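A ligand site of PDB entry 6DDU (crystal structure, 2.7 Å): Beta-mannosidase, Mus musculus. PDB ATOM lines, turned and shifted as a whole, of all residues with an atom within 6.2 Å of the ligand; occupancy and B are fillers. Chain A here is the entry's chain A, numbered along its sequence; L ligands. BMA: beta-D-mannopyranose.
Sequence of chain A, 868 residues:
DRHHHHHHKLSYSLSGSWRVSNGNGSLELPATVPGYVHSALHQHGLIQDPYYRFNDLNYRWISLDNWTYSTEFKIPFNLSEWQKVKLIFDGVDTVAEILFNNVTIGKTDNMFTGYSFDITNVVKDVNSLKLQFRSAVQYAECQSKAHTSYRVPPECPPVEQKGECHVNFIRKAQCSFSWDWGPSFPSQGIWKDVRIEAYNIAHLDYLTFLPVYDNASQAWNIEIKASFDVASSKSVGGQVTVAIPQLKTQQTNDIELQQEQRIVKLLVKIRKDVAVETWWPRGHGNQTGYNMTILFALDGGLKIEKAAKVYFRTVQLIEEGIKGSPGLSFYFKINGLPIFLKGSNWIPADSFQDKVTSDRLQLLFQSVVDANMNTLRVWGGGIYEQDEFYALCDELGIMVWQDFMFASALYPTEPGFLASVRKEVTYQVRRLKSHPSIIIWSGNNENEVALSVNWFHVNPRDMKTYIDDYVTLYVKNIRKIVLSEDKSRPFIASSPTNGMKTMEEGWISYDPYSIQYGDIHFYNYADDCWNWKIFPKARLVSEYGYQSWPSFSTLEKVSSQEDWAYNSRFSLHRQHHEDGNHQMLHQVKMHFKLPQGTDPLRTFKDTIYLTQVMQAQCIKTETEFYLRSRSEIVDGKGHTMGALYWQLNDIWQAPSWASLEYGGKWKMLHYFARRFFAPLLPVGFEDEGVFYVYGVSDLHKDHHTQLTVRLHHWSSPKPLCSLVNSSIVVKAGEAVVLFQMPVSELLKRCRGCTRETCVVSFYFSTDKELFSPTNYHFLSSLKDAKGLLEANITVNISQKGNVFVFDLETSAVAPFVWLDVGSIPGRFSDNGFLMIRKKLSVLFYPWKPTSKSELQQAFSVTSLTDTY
ND2 of Asn 445 sits at hydrogen-bond distance from O1 of the ligand, at 2.6 Å.
An oxygen (O3) of the ligand sits at hydrogen-bond distance from the indole nitrogen (NE1) of Trp 181 (3.0 Å).
The side-chain carboxylate (OE1) of Glu 446 is in hydrogen-bond range of an oxygen (O6) of the ligand, 3.4 Å away.
The side-chain carboxylate of Glu 543 is in hydrogen-bond range of an oxygen (O1) of the ligand, at 2.8 Å.
OD1 of Asp 180 is in hydrogen-bond range of O3 of the ligand, at 2.8 Å.
The indole nitrogen (NE1) of Trp 379 lies within hydrogen-bond range of an oxygen (O1) of the ligand (3.1 Å).
The indole nitrogen of Trp 179 lies within hydrogen-bond range of an oxygen (O3) of the ligand (3.0 Å).
OH of Tyr 523 touches C5 of the ligand (3.7 Å).
Trp 646 touches the ligand (CZ2 to C2, 3.5 Å).
Hydrophobic or aromatic side chains within 4 Å of the ligand: Trp 179, Trp 181, Trp 379, Tyr 523 and Trp 646.
The nearest printed residue that does not touch the ligand is Trp 657 (4.1 Å).
NH1 of Arg 377 is in salt-bridge range of OE2 of Glu 543 (2.8 Å).
The side-chain carboxylate (OE1) of Glu 446 sits at hydrogen-bond distance from the side-chain hydroxyl (OG) of Ser 408.
A ring nitrogen (ND1) of His 521 sits at hydrogen-bond distance from the side-chain carboxylate of Glu 543, at 3.1 Å.
The indole nitrogen (NE1) of Trp 646 is in hydrogen-bond range of the side-chain amide oxygen (OE1) of Gln 647, at 2.8 Å.
The side-chain carboxylate (OE2) of Glu 446 lies within hydrogen-bond range of a ring nitrogen (ND1) of His 521 (3.2 Å).
The guanidinium group of Arg 377 lies close to the side-chain amide nitrogen of Asn 445 (3.5 Å).
The indole nitrogen (NE1) of Trp 379 lies close to the side-chain amide nitrogen (ND2) of Asn 445, at 3.2 Å.
The side-chain hydroxyl of Ser 408 is in hydrogen-bond range of the side-chain amide oxygen of Asn 445, 2.6 Å away.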
ATOM      1  N   TRP A 179       7.014  -3.400  11.217  1.00  0.00           N
ATOM      2  CA  TRP A 179       7.647  -2.138  10.880  1.00  0.00           C
ATOM      3  C   TRP A 179       8.952  -2.063  11.661  1.00  0.00           C
ATOM      4  O   TRP A 179       9.299  -2.996  12.401  1.00  0.00           O
ATOM      5  CB  TRP A 179       6.722  -0.961  11.177  1.00  0.00           C
ATOM      6  CG  TRP A 179       6.904   0.210  10.262  1.00  0.00           C
ATOM      7  CD1 TRP A 179       7.611   1.353  10.531  1.00  0.00           C
ATOM      8  CD2 TRP A 179       6.387   0.359   8.936  1.00  0.00           C
ATOM      9  NE1 TRP A 179       7.560   2.198   9.449  1.00  0.00           N
ATOM     10  CE2 TRP A 179       6.816   1.611   8.461  1.00  0.00           C
ATOM     11  CE3 TRP A 179       5.602  -0.442   8.112  1.00  0.00           C
ATOM     12  CZ2 TRP A 179       6.477   2.075   7.190  1.00  0.00           C
ATOM     13  CZ3 TRP A 179       5.266   0.021   6.855  1.00  0.00           C
ATOM     14  CH2 TRP A 179       5.711   1.271   6.406  1.00  0.00           C
ATOM     15  N   ASP A 180       9.692  -0.967  11.511  1.00  0.00           N
ATOM     16  CA  ASP A 180      10.944  -0.824  12.245  1.00  0.00           C
ATOM     17  C   ASP A 180      10.724  -0.478  13.720  1.00  0.00           C
ATOM     18  O   ASP A 180      11.697  -0.162  14.415  1.00  0.00           O
ATOM     19  CB  ASP A 180      11.851   0.220  11.588  1.00  0.00           C
ATOM     20  CG  ASP A 180      11.221   1.594  11.525  1.00  0.00           C
ATOM     21  OD1 ASP A 180      10.137   1.791  12.116  1.00  0.00           O
ATOM     22  OD2 ASP A 180      11.818   2.486  10.887  1.00  0.00           O
ATOM     23  N   TRP A 181       9.480  -0.527  14.208  1.00  0.00           N
ATOM     24  CA  TRP A 181       9.196  -0.468  15.635  1.00  0.00           C
ATOM     25  C   TRP A 181       8.028  -1.342  16.052  1.00  0.00           C
ATOM     26  O   TRP A 181       7.673  -1.346  17.242  1.00  0.00           O
ATOM     27  CB  TRP A 181       8.908   0.989  16.071  1.00  0.00           C
ATOM     28  CG  TRP A 181       8.137   1.775  15.062  1.00  0.00           C
ATOM     29  CD1 TRP A 181       8.580   2.844  14.343  1.00  0.00           C
ATOM     30  CD2 TRP A 181       6.782   1.553  14.642  1.00  0.00           C
ATOM     31  NE1 TRP A 181       7.599   3.301  13.510  1.00  0.00           N
ATOM     32  CE2 TRP A 181       6.476   2.529  13.672  1.00  0.00           C
ATOM     33  CE3 TRP A 181       5.795   0.622  14.992  1.00  0.00           C
ATOM     34  CZ2 TRP A 181       5.241   2.604  13.042  1.00  0.00           C
ATOM     35  CZ3 TRP A 181       4.562   0.703  14.370  1.00  0.00           C
ATOM     36  CH2 TRP A 181       4.288   1.679  13.407  1.00  0.00           C
ATOM     37  N   ARG A 377       0.092  13.977  14.094  1.00  0.00           N
ATOM     38  CA  ARG A 377       0.068  13.501  12.711  1.00  0.00           C
ATOM     39  C   ARG A 377      -0.326  12.029  12.714  1.00  0.00           C
ATOM     40  O   ARG A 377       0.459  11.163  13.124  1.00  0.00           O
ATOM     41  CB  ARG A 377       1.433  13.702  12.044  1.00  0.00           C
ATOM     42  CG  ARG A 377       1.549  12.981  10.710  1.00  0.00           C
ATOM     43  CD  ARG A 377       2.635  13.590   9.843  1.00  0.00           C
ATOM     44  NE  ARG A 377       2.774  12.870   8.569  1.00  0.00           N
ATOM     45  CZ  ARG A 377       3.736  11.998   8.285  1.00  0.00           C
ATOM     46  NH1 ARG A 377       4.676  11.705   9.186  1.00  0.00           N
ATOM     47  NH2 ARG A 377       3.760  11.411   7.107  1.00  0.00           N
ATOM     48  N   TRP A 379      -0.126   9.044  11.285  1.00  0.00           N
ATOM     49  CA  TRP A 379       0.837   8.578  10.297  1.00  0.00           C
ATOM     50  C   TRP A 379       0.199   7.585   9.329  1.00  0.00           C
ATOM     51  O   TRP A 379      -0.552   6.693   9.732  1.00  0.00           O
ATOM     52  CB  TRP A 379       2.025   7.954  11.032  1.00  0.00           C
ATOM     53  CG  TRP A 379       3.040   7.298  10.168  1.00  0.00           C
ATOM     54  CD1 TRP A 379       3.901   7.900   9.299  1.00  0.00           C
ATOM     55  CD2 TRP A 379       3.329   5.898  10.122  1.00  0.00           C
ATOM     56  NE1 TRP A 379       4.693   6.957   8.697  1.00  0.00           N
ATOM     57  CE2 TRP A 379       4.370   5.717   9.193  1.00  0.00           C
ATOM     58  CE3 TRP A 379       2.802   4.785  10.776  1.00  0.00           C
ATOM     59  CZ2 TRP A 379       4.887   4.469   8.892  1.00  0.00           C
ATOM     60  CZ3 TRP A 379       3.321   3.542  10.483  1.00  0.00           C
ATOM     61  CH2 TRP A 379       4.360   3.398   9.550  1.00  0.00           C
ATOM     62  N   SER A 408       5.428   4.630   2.697  1.00  0.00           N
ATOM     63  CA  SER A 408       6.741   4.064   2.414  1.00  0.00           C
ATOM     64  C   SER A 408       6.647   2.833   1.516  1.00  0.00           C
ATOM     65  O   SER A 408       7.161   1.762   1.835  1.00  0.00           O
ATOM     66  CB  SER A 408       7.472   3.727   3.713  1.00  0.00           C
ATOM     67  OG  SER A 408       7.588   4.864   4.555  1.00  0.00           O
ATOM     68  N   ASN A 445       3.027   8.749   2.983  1.00  0.00           N
ATOM     69  CA  ASN A 445       4.216   8.954   3.809  1.00  0.00           C
ATOM     70  C   ASN A 445       5.453   8.550   3.006  1.00  0.00           C
ATOM     71  O   ASN A 445       5.644   7.363   2.717  1.00  0.00           O
ATOM     72  CB  ASN A 445       4.127   8.146   5.100  1.00  0.00           C
ATOM     73  CG  ASN A 445       5.486   7.874   5.714  1.00  0.00           C
ATOM     74  OD1 ASN A 445       6.080   6.809   5.507  1.00  0.00           O
ATOM     75  ND2 ASN A 445       6.007   8.843   6.473  1.00  0.00           N
ATOM     76  N   GLU A 446       6.271   9.538   2.640  1.00  0.00           N
ATOM     77  CA  GLU A 446       7.609   9.345   2.088  1.00  0.00           C
ATOM     78  C   GLU A 446       7.609   8.714   0.700  1.00  0.00           C
ATOM     79  O   GLU A 446       8.678   8.336   0.213  1.00  0.00           O
ATOM     80  CB  GLU A 446       8.476   8.497   3.012  1.00  0.00           C
ATOM     81  CG  GLU A 446       8.782   9.163   4.350  1.00  0.00           C
ATOM     82  CD  GLU A 446       9.717   8.333   5.217  1.00  0.00           C
ATOM     83  OE1 GLU A 446       9.800   7.098   4.992  1.00  0.00           O
ATOM     84  OE2 GLU A 446      10.369   8.914   6.108  1.00  0.00           O
ATOM     85  N   TRP A 455      14.325   4.790  -3.767  1.00  0.00           N
ATOM     86  CA  TRP A 455      14.668   3.888  -2.667  1.00  0.00           C
ATOM     87  C   TRP A 455      14.713   2.447  -3.136  1.00  0.00           C
ATOM     88  O   TRP A 455      15.590   1.673  -2.716  1.00  0.00           O
ATOM     89  CB  TRP A 455      13.653   4.021  -1.530  1.00  0.00           C
ATOM     90  CG  TRP A 455      13.828   5.218  -0.645  1.00  0.00           C
ATOM     91  CD1 TRP A 455      14.843   6.140  -0.675  1.00  0.00           C
ATOM     92  CD2 TRP A 455      12.955   5.621   0.419  1.00  0.00           C
ATOM     93  NE1 TRP A 455      14.645   7.079   0.304  1.00  0.00           N
ATOM     94  CE2 TRP A 455      13.501   6.792   0.988  1.00  0.00           C
ATOM     95  CE3 TRP A 455      11.771   5.106   0.945  1.00  0.00           C
ATOM     96  CZ2 TRP A 455      12.890   7.450   2.062  1.00  0.00           C
ATOM     97  CZ3 TRP A 455      11.167   5.766   2.004  1.00  0.00           C
ATOM     98  CH2 TRP A 455      11.730   6.925   2.553  1.00  0.00           C
ATOM     99  N   HIS A 521      11.701  15.386   6.588  1.00  0.00           N
ATOM    100  CA  HIS A 521      12.003  14.418   7.633  1.00  0.00           C
ATOM    101  C   HIS A 521      13.510  14.339   7.774  1.00  0.00           C
ATOM    102  O   HIS A 521      14.232  14.301   6.761  1.00  0.00           O
ATOM    103  CB  HIS A 521      11.430  13.026   7.297  1.00  0.00           C
ATOM    104  CG  HIS A 521       9.950  13.024   7.034  1.00  0.00           C
ATOM    105  ND1 HIS A 521       9.267  11.871   6.730  1.00  0.00           N
ATOM    106  CD2 HIS A 521       9.034  14.018   7.072  1.00  0.00           C
ATOM    107  CE1 HIS A 521       7.985  12.158   6.566  1.00  0.00           C
ATOM    108  NE2 HIS A 521       7.814  13.446   6.765  1.00  0.00           N
ATOM    109  N   TYR A 523      16.728  12.340   9.878  1.00  0.00           N
ATOM    110  CA  TYR A 523      17.229  11.281  10.747  1.00  0.00           C
ATOM    111  C   TYR A 523      18.743  11.195  10.588  1.00  0.00           C
ATOM    112  O   TYR A 523      19.255  11.222   9.467  1.00  0.00           O
ATOM    113  CB  TYR A 523      16.592   9.933  10.401  1.00  0.00           C
ATOM    114  CG  TYR A 523      15.124   9.858  10.702  1.00  0.00           C
ATOM    115  CD1 TYR A 523      14.672   9.610  11.985  1.00  0.00           C
ATOM    116  CD2 TYR A 523      14.174  10.039   9.699  1.00  0.00           C
ATOM    117  CE1 TYR A 523      13.323   9.543  12.269  1.00  0.00           C
ATOM    118  CE2 TYR A 523      12.823   9.980   9.976  1.00  0.00           C
ATOM    119  CZ  TYR A 523      12.404   9.731  11.267  1.00  0.00           C
ATOM    120  OH  TYR A 523      11.052   9.666  11.537  1.00  0.00           O
ATOM    121  N   TYR A 525      22.084   9.196  12.694  1.00  0.00           N
ATOM    122  CA  TYR A 525      22.544   8.338  13.772  1.00  0.00           C
ATOM    123  C   TYR A 525      24.062   8.309  13.923  1.00  0.00           C
ATOM    124  O   TYR A 525      24.561   7.711  14.878  1.00  0.00           O
ATOM    125  CB  TYR A 525      22.044   6.906  13.577  1.00  0.00           C
ATOM    126  CG  TYR A 525      20.563   6.784  13.295  1.00  0.00           C
ATOM    127  CD1 TYR A 525      19.622   7.088  14.272  1.00  0.00           C
ATOM    128  CD2 TYR A 525      20.099   6.364  12.058  1.00  0.00           C
ATOM    129  CE1 TYR A 525      18.270   6.978  14.021  1.00  0.00           C
ATOM    130  CE2 TYR A 525      18.754   6.256  11.792  1.00  0.00           C
ATOM    131  CZ  TYR A 525      17.845   6.559  12.775  1.00  0.00           C
ATOM    132  OH  TYR A 525      16.490   6.451  12.511  1.00  0.00           O
ATOM    133  N   GLU A 543       8.947  15.258  10.802  1.00  0.00           N
ATOM    134  CA  GLU A 543       9.496  14.047  11.407  1.00  0.00           C
ATOM    135  C   GLU A 543      10.935  14.308  11.790  1.00  0.00           C
ATOM    136  O   GLU A 543      11.658  15.027  11.101  1.00  0.00           O
ATOM    137  CB  GLU A 543       9.444  12.833  10.471  1.00  0.00           C
ATOM    138  CG  GLU A 543       8.123  12.093  10.433  1.00  0.00           C
ATOM    139  CD  GLU A 543       8.198  10.853   9.562  1.00  0.00           C
ATOM    140  OE1 GLU A 543       9.314  10.303   9.411  1.00  0.00           O
ATOM    141  OE2 GLU A 543       7.158  10.438   9.018  1.00  0.00           O
ATOM    142  N   HIS A 577      15.069  -2.114  13.844  1.00  0.00           N
ATOM    143  CA  HIS A 577      15.822  -1.118  13.086  1.00  0.00           C
ATOM    144  C   HIS A 577      17.242  -1.618  12.873  1.00  0.00           C
ATOM    145  O   HIS A 577      17.867  -2.128  13.808  1.00  0.00           O
ATOM    146  CB  HIS A 577      15.837   0.235  13.817  1.00  0.00           C
ATOM    147  CG  HIS A 577      16.478   1.326  13.027  1.00  0.00           C
ATOM    148  ND1 HIS A 577      15.893   1.874  11.904  1.00  0.00           N
ATOM    149  CD2 HIS A 577      17.648   1.981  13.207  1.00  0.00           C
ATOM    150  CE1 HIS A 577      16.686   2.824  11.417  1.00  0.00           C
ATOM    151  NE2 HIS A 577      17.752   2.906  12.186  1.00  0.00           N
ATOM    152  N   TRP A 646       9.365  12.354  15.744  1.00  0.00           N
ATOM    153  CA  TRP A 646       9.012  10.951  15.614  1.00  0.00           C
ATOM    154  C   TRP A 646       9.577  10.183  16.808  1.00  0.00           C
ATOM    155  O   TRP A 646      10.776  10.278  17.061  1.00  0.00           O
ATOM    156  CB  TRP A 646       9.550  10.364  14.308  1.00  0.00           C
ATOM    157  CG  TRP A 646       9.082   8.971  14.073  1.00  0.00           C
ATOM    158  CD1 TRP A 646       9.699   7.821  14.479  1.00  0.00           C
ATOM    159  CD2 TRP A 646       7.896   8.575  13.381  1.00  0.00           C
ATOM    160  NE1 TRP A 646       8.953   6.739  14.086  1.00  0.00           N
ATOM    161  CE2 TRP A 646       7.844   7.167  13.410  1.00  0.00           C
ATOM    162  CE3 TRP A 646       6.862   9.276  12.750  1.00  0.00           C
ATOM    163  CZ2 TRP A 646       6.813   6.449  12.829  1.00  0.00           C
ATOM    164  CZ3 TRP A 646       5.841   8.559  12.167  1.00  0.00           C
ATOM    165  CH2 TRP A 646       5.822   7.156  12.210  1.00  0.00           C
ATOM    166  N   GLN A 647       8.768   9.442  17.572  1.00  0.00           N
ATOM    167  CA  GLN A 647       7.325   9.302  17.419  1.00  0.00           C
ATOM    168  C   GLN A 647       6.675   9.522  18.781  1.00  0.00           C
ATOM    169  O   GLN A 647       7.374   9.796  19.764  1.00  0.00           O
ATOM    170  CB  GLN A 647       6.964   7.916  16.877  1.00  0.00           C
ATOM    171  CG  GLN A 647       7.205   6.796  17.863  1.00  0.00           C
ATOM    172  CD  GLN A 647       7.511   5.467  17.195  1.00  0.00           C
ATOM    173  OE1 GLN A 647       8.493   5.339  16.473  1.00  0.00           O
ATOM    174  NE2 GLN A 647       6.666   4.476  17.435  1.00  0.00           N
ATOM    175  N   TRP A 657      11.423   5.130  18.622  1.00  0.00           N
ATOM    176  CA  TRP A 657      11.634   6.564  18.714  1.00  0.00           C
ATOM    177  C   TRP A 657      10.606   7.244  19.613  1.00  0.00           C
ATOM    178  O   TRP A 657      10.611   8.470  19.724  1.00  0.00           O
ATOM    179  CB  TRP A 657      11.582   7.196  17.322  1.00  0.00           C
ATOM    180  CG  TRP A 657      12.629   6.669  16.382  1.00  0.00           C
ATOM    181  CD1 TRP A 657      13.801   7.272  16.049  1.00  0.00           C
ATOM    182  CD2 TRP A 657      12.594   5.428  15.666  1.00  0.00           C
ATOM    183  NE1 TRP A 657      14.498   6.489  15.170  1.00  0.00           N
ATOM    184  CE2 TRP A 657      13.784   5.345  14.917  1.00  0.00           C
ATOM    185  CE3 TRP A 657      11.681   4.374  15.589  1.00  0.00           C
ATOM    186  CZ2 TRP A 657      14.071   4.265  14.093  1.00  0.00           C
ATOM    187  CZ3 TRP A 657      11.971   3.292  14.779  1.00  0.00           C
ATOM    188  CH2 TRP A 657      13.164   3.250  14.048  1.00  0.00           C
HETATM  189  C1  BMA L   1       8.647   7.344   9.128  1.00  0.00           C
HETATM  190  C2  BMA L   1       8.272   5.988   9.653  1.00  0.00           C
HETATM  191  C3  BMA L   1       9.387   5.522  10.587  1.00  0.00           C
HETATM  192  C4  BMA L   1      10.777   5.589   9.923  1.00  0.00           C
HETATM  193  C5  BMA L   1      10.993   6.919   9.133  1.00  0.00           C
HETATM  194  C6  BMA L   1      12.162   6.837   8.148  1.00  0.00           C
HETATM  195  O1  BMA L   1       7.620   7.754   8.264  1.00  0.00           O
HETATM  196  O2  BMA L   1       8.199   5.040   8.601  1.00  0.00           O
HETATM  197  O3  BMA L   1       9.142   4.200  11.057  1.00  0.00           O
HETATM  198  O4  BMA L   1      11.768   5.492  10.940  1.00  0.00           O
HETATM  199  O5  BMA L   1       9.823   7.256   8.359  1.00  0.00           O
HETATM  200  O6  BMA L   1      11.920   5.755   7.245  1.00  0.00           O
